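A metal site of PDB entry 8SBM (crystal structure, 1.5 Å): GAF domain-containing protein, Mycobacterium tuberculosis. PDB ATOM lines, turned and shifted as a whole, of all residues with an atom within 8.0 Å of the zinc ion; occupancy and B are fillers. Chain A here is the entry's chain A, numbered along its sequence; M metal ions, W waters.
The side-chain carboxylate of Asp 68 lies within salt-bridge range of the side-chain amino group of Lys 66 (3.96 Å). The backbone carbonyl oxygen (O) of Cys 72 lies within hydrogen-bond range of the backbone NH (N) of Lys 66 (2.9 Å).
The zinc ion is bound by OD1 of Asp 70, at 2.0 Å. Water W1 is bound to the zinc ion (2.0 Å). The zinc ion is bound by OD1 of Asp 68, 2.1 Å away. The zinc ion is bound by SG of Cys 72, at 2.3 Å. The zinc ion has four donor atoms within binding distance.
Water W1 lies within hydrogen-bond range of the side-chain carboxylate (OD1) of Asp 69 (3.0 Å) and the side-chain carboxylate (OD2) of Asp 68 (3.3 Å).
Asp 69 touches the zinc ion. Within 4 Å of the zinc ion: Asp 68, Asp 69, Asp 70 and Cys 72.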
ATOM      1  N   VAL A  65       4.704 -15.905 -23.908  1.00  0.00           N
ATOM      2  CA  VAL A  65       3.686 -14.909 -24.232  1.00  0.00           C
ATOM      3  C   VAL A  65       2.344 -15.621 -24.173  1.00  0.00           C
ATOM      4  O   VAL A  65       2.116 -16.588 -24.898  1.00  0.00           O
ATOM      5  CB  VAL A  65       3.906 -14.285 -25.617  1.00  0.00           C
ATOM      6  CG1 VAL A  65       2.773 -13.319 -25.949  1.00  0.00           C
ATOM      7  CG2 VAL A  65       5.251 -13.595 -25.679  1.00  0.00           C
ATOM      8  N   LYS A  66       1.463 -15.137 -23.300  1.00  0.00           N
ATOM      9  CA  LYS A  66       0.195 -15.802 -23.042  1.00  0.00           C
ATOM     10  C   LYS A  66      -0.949 -14.813 -23.205  1.00  0.00           C
ATOM     11  O   LYS A  66      -0.868 -13.665 -22.745  1.00  0.00           O
ATOM     12  CB  LYS A  66       0.187 -16.406 -21.636  1.00  0.00           C
ATOM     13  CG  LYS A  66      -1.102 -17.098 -21.240  1.00  0.00           C
ATOM     14  CD  LYS A  66      -0.876 -18.004 -20.024  1.00  0.00           C
ATOM     15  CE  LYS A  66      -0.197 -17.253 -18.891  1.00  0.00           C
ATOM     16  NZ  LYS A  66       0.007 -18.107 -17.685  1.00  0.00           N
ATOM     17  N   VAL A  67      -2.008 -15.248 -23.879  1.00  0.00           N
ATOM     18  CA  VAL A  67      -3.239 -14.478 -23.974  1.00  0.00           C
ATOM     19  C   VAL A  67      -4.307 -15.288 -23.264  1.00  0.00           C
ATOM     20  O   VAL A  67      -4.690 -16.374 -23.724  1.00  0.00           O
ATOM     21  CB  VAL A  67      -3.619 -14.193 -25.429  1.00  0.00           C
ATOM     22  CG1 VAL A  67      -4.988 -13.529 -25.515  1.00  0.00           C
ATOM     23  CG2 VAL A  67      -2.557 -13.318 -26.079  1.00  0.00           C
ATOM     24  N   ASP A  68      -4.759 -14.781 -22.115  1.00  0.00           N
ATOM     25  CA  ASP A  68      -5.805 -15.431 -21.340  1.00  0.00           C
ATOM     26  C   ASP A  68      -6.870 -14.404 -20.981  1.00  0.00           C
ATOM     27  O   ASP A  68      -7.565 -13.889 -21.857  1.00  0.00           O
ATOM     28  CB  ASP A  68      -5.240 -16.133 -20.104  1.00  0.00           C
ATOM     29  CG  ASP A  68      -4.013 -15.418 -19.507  1.00  0.00           C
ATOM     30  OD1 ASP A  68      -3.866 -14.182 -19.657  1.00  0.00           O
ATOM     31  OD2 ASP A  68      -3.201 -16.109 -18.874  1.00  0.00           O
ATOM     32  N   ASP A  69      -6.989 -14.063 -19.697  1.00  0.00           N
ATOM     33  CA  ASP A  69      -7.820 -12.935 -19.323  1.00  0.00           C
ATOM     34  C   ASP A  69      -7.215 -11.626 -19.814  1.00  0.00           C
ATOM     35  O   ASP A  69      -7.947 -10.647 -20.042  1.00  0.00           O
ATOM     36  CB  ASP A  69      -8.019 -12.892 -17.804  1.00  0.00           C
ATOM     37  CG  ASP A  69      -6.702 -12.878 -17.054  1.00  0.00           C
ATOM     38  OD1 ASP A  69      -5.932 -13.845 -17.177  1.00  0.00           O
ATOM     39  OD2 ASP A  69      -6.441 -11.879 -16.351  1.00  0.00           O
ATOM     40  N   ASP A  70      -5.897 -11.593 -19.974  1.00  0.00           N
ATOM     41  CA  ASP A  70      -5.171 -10.405 -20.423  1.00  0.00           C
ATOM     42  C   ASP A  70      -4.081 -10.855 -21.393  1.00  0.00           C
ATOM     43  O   ASP A  70      -4.067 -12.000 -21.849  1.00  0.00           O
ATOM     44  CB  ASP A  70      -4.605  -9.649 -19.211  1.00  0.00           C
ATOM     45  CG  ASP A  70      -3.630 -10.494 -18.393  1.00  0.00           C
ATOM     46  OD1 ASP A  70      -3.235 -11.588 -18.854  1.00  0.00           O
ATOM     47  OD2 ASP A  70      -3.257 -10.064 -17.279  1.00  0.00           O
ATOM     48  N   LEU A  71      -3.176  -9.943 -21.715  1.00  0.00           N
ATOM     49  CA  LEU A  71      -1.917 -10.293 -22.370  1.00  0.00           C
ATOM     50  C   LEU A  71      -0.826 -10.269 -21.317  1.00  0.00           C
ATOM     51  O   LEU A  71      -0.659  -9.260 -20.619  1.00  0.00           O
ATOM     52  CB  LEU A  71      -1.575  -9.293 -23.471  1.00  0.00           C
ATOM     53  CG  LEU A  71      -0.154  -9.490 -24.002  1.00  0.00           C
ATOM     54  CD1 LEU A  71      -0.059 -10.770 -24.814  1.00  0.00           C
ATOM     55  CD2 LEU A  71       0.321  -8.301 -24.824  1.00  0.00           C
ATOM     56  N   CYS A  72      -0.078 -11.356 -21.188  1.00  0.00           N
ATOM     57  CA  CYS A  72       1.003 -11.374 -20.220  1.00  0.00           C
ATOM     58  C   CYS A  72       2.247 -12.021 -20.797  1.00  0.00           C
ATOM     59  O   CYS A  72       2.196 -13.058 -21.470  1.00  0.00           O
ATOM     60  CB  CYS A  72       0.588 -12.032 -18.886  1.00  0.00           C
ATOM     61  SG  CYS A  72      -0.064 -13.695 -19.013  1.00  0.00           S
ATOM     62  N   ILE A  73       3.382 -11.387 -20.524  1.00  0.00           N
ATOM     63  CA  ILE A  73       4.698 -11.793 -21.011  1.00  0.00           C
ATOM     64  C   ILE A  73       5.547 -12.114 -19.788  1.00  0.00           C
ATOM     65  O   ILE A  73       5.622 -11.309 -18.855  1.00  0.00           O
ATOM     66  CB  ILE A  73       5.351 -10.652 -21.801  1.00  0.00           C
ATOM     67  CG1 ILE A  73       4.452 -10.248 -22.966  1.00  0.00           C
ATOM     68  CG2 ILE A  73       6.738 -11.059 -22.285  1.00  0.00           C
ATOM     69  CD1 ILE A  73       4.855  -8.980 -23.613  1.00  0.00           C
ATOM     70  N   ARG A 119       7.798  -9.974 -15.530  1.00  0.00           N
ATOM     71  CA  ARG A 119       6.432 -10.226 -15.936  1.00  0.00           C
ATOM     72  C   ARG A 119       5.785  -8.893 -16.290  1.00  0.00           C
ATOM     73  O   ARG A 119       5.803  -7.953 -15.489  1.00  0.00           O
ATOM     74  CB  ARG A 119       5.649 -10.935 -14.819  1.00  0.00           C
ATOM     75  CG  ARG A 119       4.436 -11.687 -15.282  1.00  0.00           C
ATOM     76  CD  ARG A 119       3.717 -12.333 -14.102  1.00  0.00           C
ATOM     77  NE  ARG A 119       4.656 -12.883 -13.135  1.00  0.00           N
ATOM     78  CZ  ARG A 119       5.115 -14.129 -13.153  1.00  0.00           C
ATOM     79  NH1 ARG A 119       4.759 -14.981 -14.100  1.00  0.00           N
ATOM     80  NH2 ARG A 119       5.963 -14.519 -12.204  1.00  0.00           N
ATOM     81  N   TRP A 120       5.245  -8.806 -17.492  1.00  0.00           N
ATOM     82  CA  TRP A 120       4.589  -7.600 -17.980  1.00  0.00           C
ATOM     83  C   TRP A 120       3.211  -8.014 -18.465  1.00  0.00           C
ATOM     84  O   TRP A 120       3.095  -8.971 -19.237  1.00  0.00           O
ATOM     85  CB  TRP A 120       5.410  -7.016 -19.141  1.00  0.00           C
ATOM     86  CG  TRP A 120       5.008  -5.638 -19.585  1.00  0.00           C
ATOM     87  CD1 TRP A 120       5.608  -4.469 -19.234  1.00  0.00           C
ATOM     88  CD2 TRP A 120       3.942  -5.295 -20.488  1.00  0.00           C
ATOM     89  NE1 TRP A 120       4.969  -3.413 -19.844  1.00  0.00           N
ATOM     90  CE2 TRP A 120       3.951  -3.894 -20.626  1.00  0.00           C
ATOM     91  CE3 TRP A 120       2.991  -6.040 -21.191  1.00  0.00           C
ATOM     92  CZ2 TRP A 120       3.036  -3.219 -21.423  1.00  0.00           C
ATOM     93  CZ3 TRP A 120       2.077  -5.365 -21.989  1.00  0.00           C
ATOM     94  CH2 TRP A 120       2.114  -3.967 -22.095  1.00  0.00           C
ATOM     95  N   SER A 121       2.172  -7.325 -18.015  1.00  0.00           N
ATOM     96  CA  SER A 121       0.824  -7.678 -18.423  1.00  0.00           C
ATOM     97  C   SER A 121       0.031  -6.422 -18.720  1.00  0.00           C
ATOM     98  O   SER A 121       0.333  -5.334 -18.215  1.00  0.00           O
ATOM     99  CB  SER A 121       0.099  -8.550 -17.382  1.00  0.00           C
ATOM    100  OG  SER A 121      -0.096  -7.852 -16.168  1.00  0.00           O
ATOM    101  N   ALA A 122      -0.991  -6.575 -19.559  1.00  0.00           N
ATOM    102  CA  ALA A 122      -1.861  -5.460 -19.874  1.00  0.00           C
ATOM    103  C   ALA A 122      -3.236  -6.010 -20.227  1.00  0.00           C
ATOM    104  O   ALA A 122      -3.332  -7.135 -20.744  1.00  0.00           O
ATOM    105  CB  ALA A 122      -1.313  -4.632 -21.049  1.00  0.00           C
ATOM    106  N   LEU A 124      -6.666  -6.673 -22.274  1.00  0.00           N
ATOM    107  CA  LEU A 124      -7.157  -6.632 -23.640  1.00  0.00           C
ATOM    108  C   LEU A 124      -8.377  -5.729 -23.689  1.00  0.00           C
ATOM    109  O   LEU A 124      -9.185  -5.701 -22.763  1.00  0.00           O
ATOM    110  CB  LEU A 124      -7.561  -8.037 -24.086  1.00  0.00           C
ATOM    111  CG  LEU A 124      -6.524  -9.134 -23.873  1.00  0.00           C
ATOM    112  CD1 LEU A 124      -7.183 -10.498 -23.949  1.00  0.00           C
ATOM    113  CD2 LEU A 124      -5.418  -9.024 -24.896  1.00  0.00           C
HETATM  114 ZN    ZN M   1      -2.332 -13.347 -18.553  1.00  0.00          ZN
HETATM  115  O   HOH W   1      -3.030 -13.607 -16.678  1.00  0.00           O
